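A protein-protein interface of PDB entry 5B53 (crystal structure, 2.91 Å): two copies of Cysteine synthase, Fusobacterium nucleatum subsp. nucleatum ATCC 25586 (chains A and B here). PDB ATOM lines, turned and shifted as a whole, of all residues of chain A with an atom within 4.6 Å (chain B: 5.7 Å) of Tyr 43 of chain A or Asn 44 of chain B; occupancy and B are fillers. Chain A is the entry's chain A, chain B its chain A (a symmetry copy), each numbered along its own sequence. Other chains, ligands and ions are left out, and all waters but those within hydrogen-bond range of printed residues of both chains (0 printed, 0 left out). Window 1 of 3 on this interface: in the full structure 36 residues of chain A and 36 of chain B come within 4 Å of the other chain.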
ATOM      1  N   GLY A  18      23.763  -9.649  12.235  1.00  0.00           N
ATOM      2  CA  GLY A  18      22.423  -9.476  12.722  1.00  0.00           C
ATOM      3  C   GLY A  18      21.337  -9.586  11.673  1.00  0.00           C
ATOM      4  O   GLY A  18      21.528 -10.086  10.544  1.00  0.00           O
ATOM      5  N   THR A  20      18.731 -11.432  11.621  1.00  0.00           N
ATOM      6  CA  THR A  20      18.457 -12.796  11.234  1.00  0.00           C
ATOM      7  C   THR A  20      17.002 -13.254  11.316  1.00  0.00           C
ATOM      8  O   THR A  20      16.187 -12.669  11.996  1.00  0.00           O
ATOM      9  CB  THR A  20      19.245 -13.700  12.158  1.00  0.00           C
ATOM     10  OG1 THR A  20      18.875 -13.443  13.527  1.00  0.00           O
ATOM     11  CG2 THR A  20      20.734 -13.439  11.930  1.00  0.00           C
ATOM     12  N   PRO A  21      16.677 -14.352  10.644  1.00  0.00           N
ATOM     13  CA  PRO A  21      15.301 -14.796  10.728  1.00  0.00           C
ATOM     14  C   PRO A  21      14.858 -15.233  12.143  1.00  0.00           C
ATOM     15  O   PRO A  21      15.630 -15.854  12.875  1.00  0.00           O
ATOM     16  CB  PRO A  21      15.270 -15.994   9.780  1.00  0.00           C
ATOM     17  CG  PRO A  21      16.465 -15.910   8.924  1.00  0.00           C
ATOM     18  CD  PRO A  21      17.473 -15.177   9.712  1.00  0.00           C
ATOM     19  N   ASN A  40      17.540 -17.607  14.123  1.00  0.00           N
ATOM     20  CA  ASN A  40      18.498 -18.420  13.418  1.00  0.00           C
ATOM     21  C   ASN A  40      19.744 -17.621  13.126  1.00  0.00           C
ATOM     22  O   ASN A  40      19.761 -16.761  12.276  1.00  0.00           O
ATOM     23  CB  ASN A  40      17.867 -18.957  12.160  1.00  0.00           C
ATOM     24  CG  ASN A  40      18.722 -19.968  11.476  1.00  0.00           C
ATOM     25  OD1 ASN A  40      19.946 -19.864  11.543  1.00  0.00           O
ATOM     26  ND2 ASN A  40      18.095 -20.939  10.771  1.00  0.00           N
ATOM     27  N   GLU A  41      20.800 -17.942  13.841  1.00  0.00           N
ATOM     28  CA  GLU A  41      21.991 -17.149  13.833  1.00  0.00           C
ATOM     29  C   GLU A  41      23.039 -17.581  12.853  1.00  0.00           C
ATOM     30  O   GLU A  41      24.132 -17.016  12.865  1.00  0.00           O
ATOM     31  CB  GLU A  41      22.603 -17.128  15.245  1.00  0.00           C
ATOM     32  CG  GLU A  41      21.792 -16.274  16.186  1.00  0.00           C
ATOM     33  CD  GLU A  41      21.425 -14.906  15.579  1.00  0.00           C
ATOM     34  OE1 GLU A  41      22.356 -14.196  15.035  1.00  0.00           O
ATOM     35  OE2 GLU A  41      20.206 -14.544  15.654  1.00  0.00           O
ATOM     36  N   SER A  42      22.779 -18.582  12.024  1.00  0.00           N
ATOM     37  CA  SER A  42      23.760 -18.870  10.962  1.00  0.00           C
ATOM     38  C   SER A  42      23.880 -17.676   9.986  1.00  0.00           C
ATOM     39  O   SER A  42      24.942 -17.374   9.490  1.00  0.00           O
ATOM     40  CB  SER A  42      23.467 -20.174  10.230  1.00  0.00           C
ATOM     41  OG  SER A  42      22.213 -20.116   9.635  1.00  0.00           O
ATOM     42  N   TYR A  43      22.801 -16.936   9.822  1.00  0.00           N
ATOM     43  CA  TYR A  43      22.748 -15.804   8.914  1.00  0.00           C
ATOM     44  C   TYR A  43      23.616 -14.596   9.336  1.00  0.00           C
ATOM     45  O   TYR A  43      23.116 -13.457   9.465  1.00  0.00           O
ATOM     46  CB  TYR A  43      21.315 -15.359   8.815  1.00  0.00           C
ATOM     47  CG  TYR A  43      20.382 -16.299   8.080  1.00  0.00           C
ATOM     48  CD1 TYR A  43      19.909 -17.470   8.684  1.00  0.00           C
ATOM     49  CD2 TYR A  43      19.903 -15.969   6.821  1.00  0.00           C
ATOM     50  CE1 TYR A  43      19.002 -18.303   8.035  1.00  0.00           C
ATOM     51  CE2 TYR A  43      18.994 -16.764   6.182  1.00  0.00           C
ATOM     52  CZ  TYR A  43      18.540 -17.941   6.786  1.00  0.00           C
ATOM     53  OH  TYR A  43      17.612 -18.725   6.145  1.00  0.00           O
ATOM     54  N   ASN A  44      24.914 -14.859   9.475  1.00  0.00           N
ATOM     55  CA  ASN A  44      25.902 -13.924   9.925  1.00  0.00           C
ATOM     56  C   ASN A  44      27.230 -14.245   9.238  1.00  0.00           C
ATOM     57  O   ASN A  44      27.451 -15.332   8.703  1.00  0.00           O
ATOM     58  CB  ASN A  44      26.138 -14.167  11.415  1.00  0.00           C
ATOM     59  CG  ASN A  44      25.153 -13.466  12.322  1.00  0.00           C
ATOM     60  OD1 ASN A  44      25.080 -12.230  12.339  1.00  0.00           O
ATOM     61  ND2 ASN A  44      24.456 -14.246  13.158  1.00  0.00           N
ATOM     62  N   ARG A 338      11.543 -11.122   9.903  1.00  0.00           N
ATOM     63  CA  ARG A 338      12.886 -10.640   9.605  1.00  0.00           C
ATOM     64  C   ARG A 338      12.655  -9.220   9.345  1.00  0.00           C
ATOM     65  O   ARG A 338      11.714  -8.935   8.713  1.00  0.00           O
ATOM     66  CB  ARG A 338      13.435 -11.341   8.349  1.00  0.00           C
ATOM     67  CG  ARG A 338      14.907 -11.102   8.115  1.00  0.00           C
ATOM     68  CD  ARG A 338      15.610 -12.379   7.731  1.00  0.00           C
ATOM     69  NE  ARG A 338      17.036 -12.160   7.511  1.00  0.00           N
ATOM     70  CZ  ARG A 338      17.783 -12.755   6.578  1.00  0.00           C
ATOM     71  NH1 ARG A 338      17.279 -13.612   5.709  1.00  0.00           N
ATOM     72  NH2 ARG A 338      19.065 -12.448   6.467  1.00  0.00           N
ATOM     73  N   ASN B  15      11.505 -15.058   3.422  1.00  0.00           N
ATOM     74  CA  ASN B  15      12.383 -14.489   4.439  1.00  0.00           C
ATOM     75  C   ASN B  15      13.607 -15.285   4.865  1.00  0.00           C
ATOM     76  O   ASN B  15      14.461 -14.745   5.571  1.00  0.00           O
ATOM     77  CB  ASN B  15      11.617 -14.207   5.711  1.00  0.00           C
ATOM     78  CG  ASN B  15      10.745 -13.002   5.622  1.00  0.00           C
ATOM     79  OD1 ASN B  15       9.828 -12.893   6.427  1.00  0.00           O
ATOM     80  ND2 ASN B  15      10.993 -12.094   4.642  1.00  0.00           N
ATOM     81  N   LEU B  16      13.687 -16.561   4.482  1.00  0.00           N
ATOM     82  CA  LEU B  16      14.854 -17.387   4.766  1.00  0.00           C
ATOM     83  C   LEU B  16      15.854 -17.302   3.635  1.00  0.00           C
ATOM     84  O   LEU B  16      16.887 -17.914   3.700  1.00  0.00           O
ATOM     85  CB  LEU B  16      14.431 -18.816   4.953  1.00  0.00           C
ATOM     86  CG  LEU B  16      13.371 -19.013   6.010  1.00  0.00           C
ATOM     87  CD1 LEU B  16      12.923 -20.445   5.977  1.00  0.00           C
ATOM     88  CD2 LEU B  16      13.875 -18.662   7.391  1.00  0.00           C
ATOM     89  N   VAL B  17      15.551 -16.532   2.604  1.00  0.00           N
ATOM     90  CA  VAL B  17      16.536 -16.330   1.553  1.00  0.00           C
ATOM     91  C   VAL B  17      16.634 -14.923   0.985  1.00  0.00           C
ATOM     92  O   VAL B  17      15.641 -14.181   0.922  1.00  0.00           O
ATOM     93  CB  VAL B  17      16.285 -17.262   0.349  1.00  0.00           C
ATOM     94  CG1 VAL B  17      16.014 -18.680   0.857  1.00  0.00           C
ATOM     95  CG2 VAL B  17      15.146 -16.742  -0.535  1.00  0.00           C
ATOM     96  N   GLY B  18      17.841 -14.602   0.528  1.00  0.00           N
ATOM     97  CA  GLY B  18      18.130 -13.317  -0.044  1.00  0.00           C
ATOM     98  C   GLY B  18      18.521 -12.243   0.949  1.00  0.00           C
ATOM     99  O   GLY B  18      18.871 -12.493   2.122  1.00  0.00           O
ATOM    100  N   THR B  20      21.094 -10.351   0.998  1.00  0.00           N
ATOM    101  CA  THR B  20      22.451 -10.489   1.472  1.00  0.00           C
ATOM    102  C   THR B  20      23.352  -9.262   1.346  1.00  0.00           C
ATOM    103  O   THR B  20      23.094  -8.360   0.579  1.00  0.00           O
ATOM    104  CB  THR B  20      23.107 -11.590   0.666  1.00  0.00           C
ATOM    105  OG1 THR B  20      23.057 -11.265  -0.737  1.00  0.00           O
ATOM    106  CG2 THR B  20      22.374 -12.900   0.956  1.00  0.00           C
ATOM    107  N   ASN B  40      27.456 -11.352  -1.084  1.00  0.00           N
ATOM    108  CA  ASN B  40      27.882 -12.460  -0.266  1.00  0.00           C
ATOM    109  C   ASN B  40      26.713 -13.366   0.032  1.00  0.00           C
ATOM    110  O   ASN B  40      25.847 -13.047   0.813  1.00  0.00           O
ATOM    111  CB  ASN B  40      28.521 -11.933   0.992  1.00  0.00           C
ATOM    112  CG  ASN B  40      29.168 -13.008   1.798  1.00  0.00           C
ATOM    113  OD1 ASN B  40      28.684 -14.139   1.792  1.00  0.00           O
ATOM    114  ND2 ASN B  40      30.247 -12.664   2.540  1.00  0.00           N
ATOM    115  N   GLU B  41      26.721 -14.521  -0.597  1.00  0.00           N
ATOM    116  CA  GLU B  41      25.591 -15.399  -0.584  1.00  0.00           C
ATOM    117  C   GLU B  41      25.613 -16.451   0.483  1.00  0.00           C
ATOM    118  O   GLU B  41      24.731 -17.309   0.488  1.00  0.00           O
ATOM    119  CB  GLU B  41      25.455 -16.080  -1.957  1.00  0.00           C
ATOM    120  CG  GLU B  41      24.957 -15.117  -3.004  1.00  0.00           C
ATOM    121  CD  GLU B  41      23.745 -14.295  -2.526  1.00  0.00           C
ATOM    122  OE1 GLU B  41      22.747 -14.911  -1.987  1.00  0.00           O
ATOM    123  OE2 GLU B  41      23.794 -13.033  -2.696  1.00  0.00           O
ATOM    124  N   SER B  42      26.597 -16.455   1.371  1.00  0.00           N
ATOM    125  CA  SER B  42      26.498 -17.392   2.505  1.00  0.00           C
ATOM    126  C   SER B  42      25.276 -17.056   3.391  1.00  0.00           C
ATOM    127  O   SER B  42      24.625 -17.929   3.921  1.00  0.00           O
ATOM    128  CB  SER B  42      27.785 -17.467   3.318  1.00  0.00           C
ATOM    129  OG  SER B  42      28.096 -16.217   3.836  1.00  0.00           O
ATOM    130  N   TYR B  43      24.910 -15.790   3.438  1.00  0.00           N
ATOM    131  CA  TYR B  43      23.805 -15.315   4.251  1.00  0.00           C
ATOM    132  C   TYR B  43      22.409 -15.791   3.787  1.00  0.00           C
ATOM    133  O   TYR B  43      21.497 -14.970   3.543  1.00  0.00           O
ATOM    134  CB  TYR B  43      23.834 -13.812   4.237  1.00  0.00           C
ATOM    135  CG  TYR B  43      24.980 -13.168   4.988  1.00  0.00           C
ATOM    136  CD1 TYR B  43      26.272 -13.133   4.451  1.00  0.00           C
ATOM    137  CD2 TYR B  43      24.750 -12.513   6.190  1.00  0.00           C
ATOM    138  CE1 TYR B  43      27.312 -12.486   5.112  1.00  0.00           C
ATOM    139  CE2 TYR B  43      25.756 -11.853   6.837  1.00  0.00           C
ATOM    140  CZ  TYR B  43      27.047 -11.839   6.301  1.00  0.00           C
ATOM    141  OH  TYR B  43      28.049 -11.157   6.949  1.00  0.00           O
ATOM    142  N   ASN B  44      22.253 -17.112   3.740  1.00  0.00           N
ATOM    143  CA  ASN B  44      21.079 -17.789   3.275  1.00  0.00           C
ATOM    144  C   ASN B  44      20.922 -19.094   4.058  1.00  0.00           C
ATOM    145  O   ASN B  44      21.851 -19.603   4.686  1.00  0.00           O
ATOM    146  CB  ASN B  44      21.317 -18.204   1.824  1.00  0.00           C
ATOM    147  CG  ASN B  44      21.016 -17.122   0.812  1.00  0.00           C
ATOM    148  OD1 ASN B  44      19.871 -16.666   0.696  1.00  0.00           O
ATOM    149  ND2 ASN B  44      22.023 -16.770   0.002  1.00  0.00           N
ATOM    150  N   LEU B  45      19.753 -19.683   3.917  1.00  0.00           N
ATOM    151  CA  LEU B  45      19.323 -20.831   4.732  1.00  0.00           C
ATOM    152  C   LEU B  45      20.297 -22.000   4.789  1.00  0.00           C
ATOM    153  O   LEU B  45      20.401 -22.619   5.829  1.00  0.00           O
ATOM    154  CB  LEU B  45      17.951 -21.373   4.241  1.00  0.00           C
ATOM    155  CG  LEU B  45      17.396 -22.610   4.963  1.00  0.00           C
ATOM    156  CD1 LEU B  45      16.665 -22.222   6.229  1.00  0.00           C
ATOM    157  CD2 LEU B  45      16.443 -23.360   4.060  1.00  0.00           C
ATOM    158  N   THR B  46      20.930 -22.372   3.683  1.00  0.00           N
ATOM    159  CA  THR B  46      21.921 -23.427   3.757  1.00  0.00           C
ATOM    160  C   THR B  46      23.289 -22.921   3.344  1.00  0.00           C
ATOM    161  O   THR B  46      24.219 -23.735   3.127  1.00  0.00           O
ATOM    162  CB  THR B  46      21.539 -24.627   2.909  1.00  0.00           C
ATOM    163  OG1 THR B  46      21.338 -24.266   1.519  1.00  0.00           O
ATOM    164  CG2 THR B  46      20.299 -25.218   3.427  1.00  0.00           C
ATOM    165  N   GLY B  47      23.379 -21.579   3.186  1.00  0.00           N
ATOM    166  CA  GLY B  47      24.651 -20.852   3.046  1.00  0.00           C
ATOM    167  C   GLY B  47      25.143 -20.672   1.629  1.00  0.00           C
ATOM    168  O   GLY B  47      26.335 -20.398   1.414  1.00  0.00           O
ATOM    169  N   SER B  48      24.262 -20.853   0.657  1.00  0.00           N
ATOM    170  CA  SER B  48      24.653 -20.556  -0.681  1.00  0.00           C
ATOM    171  C   SER B  48      23.548 -19.909  -1.442  1.00  0.00           C
ATOM    172  O   SER B  48      22.391 -19.810  -0.993  1.00  0.00           O
ATOM    173  CB  SER B  48      25.106 -21.795  -1.428  1.00  0.00           C
ATOM    174  OG  SER B  48      24.016 -22.457  -2.042  1.00  0.00           O
ATOM    175  N   ILE B  49      23.964 -19.464  -2.620  1.00  0.00           N
ATOM    176  CA  ILE B  49      23.110 -18.788  -3.614  1.00  0.00           C
ATOM    177  C   ILE B  49      22.025 -19.726  -4.162  1.00  0.00           C
ATOM    178  O   ILE B  49      20.991 -19.279  -4.650  1.00  0.00           O
ATOM    179  CB  ILE B  49      23.989 -18.276  -4.793  1.00  0.00           C
ATOM    180  CG1 ILE B  49      23.217 -17.256  -5.623  1.00  0.00           C
ATOM    181  CG2 ILE B  49      24.452 -19.433  -5.607  1.00  0.00           C
ATOM    182  CD1 ILE B  49      24.093 -16.370  -6.474  1.00  0.00           C
ATOM    183  N   ASP B  51      20.122 -21.460  -2.563  1.00  0.00           N
ATOM    184  CA  ASP B  51      18.915 -21.361  -1.786  1.00  0.00           C
ATOM    185  C   ASP B  51      17.864 -20.479  -2.502  1.00  0.00           C
ATOM    186  O   ASP B  51      16.681 -20.803  -2.548  1.00  0.00           O
ATOM    187  CB  ASP B  51      19.234 -20.792  -0.393  1.00  0.00           C
ATOM    188  CG  ASP B  51      19.916 -21.790   0.518  1.00  0.00           C
ATOM    189  OD1 ASP B  51      19.553 -22.984   0.402  1.00  0.00           O
ATOM    190  OD2 ASP B  51      20.775 -21.379   1.359  1.00  0.00           O
ATOM    191  N   ARG B  52      18.294 -19.346  -3.035  1.00  0.00           N
ATOM    192  CA  ARG B  52      17.385 -18.448  -3.738  1.00  0.00           C
ATOM    193  C   ARG B  52      16.673 -19.194  -4.862  1.00  0.00           C
ATOM    194  O   ARG B  52      15.537 -18.882  -5.256  1.00  0.00           O
ATOM    195  CB  ARG B  52      18.157 -17.304  -4.363  1.00  0.00           C
ATOM    196  CG  ARG B  52      18.786 -16.389  -3.353  1.00  0.00           C
ATOM    197  CD  ARG B  52      19.523 -15.308  -4.087  1.00  0.00           C
ATOM    198  NE  ARG B  52      20.264 -14.325  -3.279  1.00  0.00           N
ATOM    199  CZ  ARG B  52      19.803 -13.131  -2.953  1.00  0.00           C
ATOM    200  NH1 ARG B  52      18.562 -12.791  -3.275  1.00  0.00           N
ATOM    201  NH2 ARG B  52      20.580 -12.296  -2.290  1.00  0.00           N
ATOM    202  N   ARG B 338      22.991  -3.319   2.286  1.00  0.00           N
ATOM    203  CA  ARG B 338      22.091  -4.415   2.620  1.00  0.00           C
ATOM    204  C   ARG B 338      20.806  -3.732   2.757  1.00  0.00           C
ATOM    205  O   ARG B 338      20.801  -2.704   3.312  1.00  0.00           O
ATOM    206  CB  ARG B 338      22.510  -5.059   3.954  1.00  0.00           C
ATOM    207  CG  ARG B 338      21.803  -6.359   4.251  1.00  0.00           C
ATOM    208  CD  ARG B 338      22.767  -7.395   4.770  1.00  0.00           C
ATOM    209  NE  ARG B 338      22.094  -8.659   5.051  1.00  0.00           N
ATOM    210  CZ  ARG B 338      22.368  -9.481   6.067  1.00  0.00           C
ATOM    211  NH1 ARG B 338      23.291  -9.206   6.970  1.00  0.00           N
ATOM    212  NH2 ARG B 338      21.664 -10.589   6.226  1.00  0.00           N
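The side-chain hydroxyl (OH) of Tyr 43 of chain A sits at hydrogen-bond distance from the backbone carbonyl oxygen (O) of Leu 16 of chain B.
NH2 of Arg 338 of chain A lies close to NH2 of Arg 338 of chain B, 3.2 Å away.
O of Asn 15 of chain B is in hydrogen-bond range of NH1 of Arg 338 of chain A, 3.0 Å away.
N of Leu 45 of chain B lies close to OH of Tyr 43 of chain A (3.2 Å).
The backbone NH (N) of Leu 45 of chain B lies within hydrogen-bond range of the side-chain carboxylate (OD2) of Asp 51 of chain B (3.2 Å).
N of Gly 18 of chain A sits at hydrogen-bond distance from OD1 of Asn 44 of chain A, 2.9 Å away.
The backbone carbonyl oxygen (O) of Pro 21 of chain A is in hydrogen-bond range of the backbone NH (N) of Asn 40 of chain A (2.9 Å).
The backbone carbonyl oxygen (O) of Glu 41 of chain A sits at hydrogen-bond distance from the side-chain amide nitrogen (ND2) of Asn 44 of chain A (2.8 Å).
The backbone NH of Gly 18 of chain B lies within hydrogen-bond range of the side-chain amide oxygen of Asn 44 of chain B (2.9 Å).
The side-chain amide nitrogen (ND2) of Asn 44 of chain B lies within hydrogen-bond range of the backbone carbonyl oxygen (O) of Ser 48 of chain B (3.2 Å).
Among the printed residues, merely in contact across the chains: Tyr 43 of chain A with Asn 44 of chain B (3.7 Å), Asn 44 of chain A with Tyr 43 of chain B (3.7 Å), Tyr 43 of chain A with Tyr 43 of chain B (3.8 Å) and Pro 21 of chain A with Leu 16 of chain B (3.8 Å).
Of the printed residues of chain B, Pro 21 of chain A touches Leu 16.
Tyr 43 of chain A touches just these residues of chain B: Leu 16, Tyr 43, Asn 44 and Leu 45.
Of the printed residues of chain A, Leu 16 of chain B touches Pro 21 and Tyr 43.
Printed residues of chain A within 4 Å of Tyr 43 of chain B: Tyr 43 and Asn 44.
Of chain A, only Tyr 43 (3.7 Å) comes within 4 Å of Asn 44 of chain B.
Printed residues of chain A within 4 Å of Leu 45 of chain B: Tyr 43.
Gly 47 of chain B touches none of the printed residues of chain A.
The nearest residue of chain B that does not touch Tyr 43 of chain A is Arg 338 of chain B (4.6 Å).
Of the 9 printed residues of chain A, 4 touch a printed residue of chain B.
Printed residues of chain A that touch a printed residue of chain B: Pro 21, Tyr 43, Asn 44 and Arg 338.
Hydrophobic or aromatic side chains of chain A within 4 Å of the printed part of chain B: Pro 21 and Tyr 43.
Printed residues of chain B that touch a printed residue of chain A: Asn 15, Leu 16, Tyr 43, Asn 44, Leu 45 and Arg 338.
Hydrophobic or aromatic side chains of chain B within 4 Å of the printed part of chain A: Leu 16, Tyr 43 and Leu 45.
Among the printed residues, no Asp or Glu carboxylate lies within 4 Å of a Lys or Arg side-chain nitrogen of the other chain.
Tyr 43 of chain A touches its own counterpart, Tyr 43 of chain B.
Tyr 43 of chain A touches Asn 44 of chain B, and with the chains exchanged Asn 44 of chain A touches Tyr 43 of chain B.
Arg 338 of chain A touches its own counterpart, Arg 338 of chain B.
Positions printed for both chains: 18, 20, 40, 41, 42, 43, 44 and 338.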
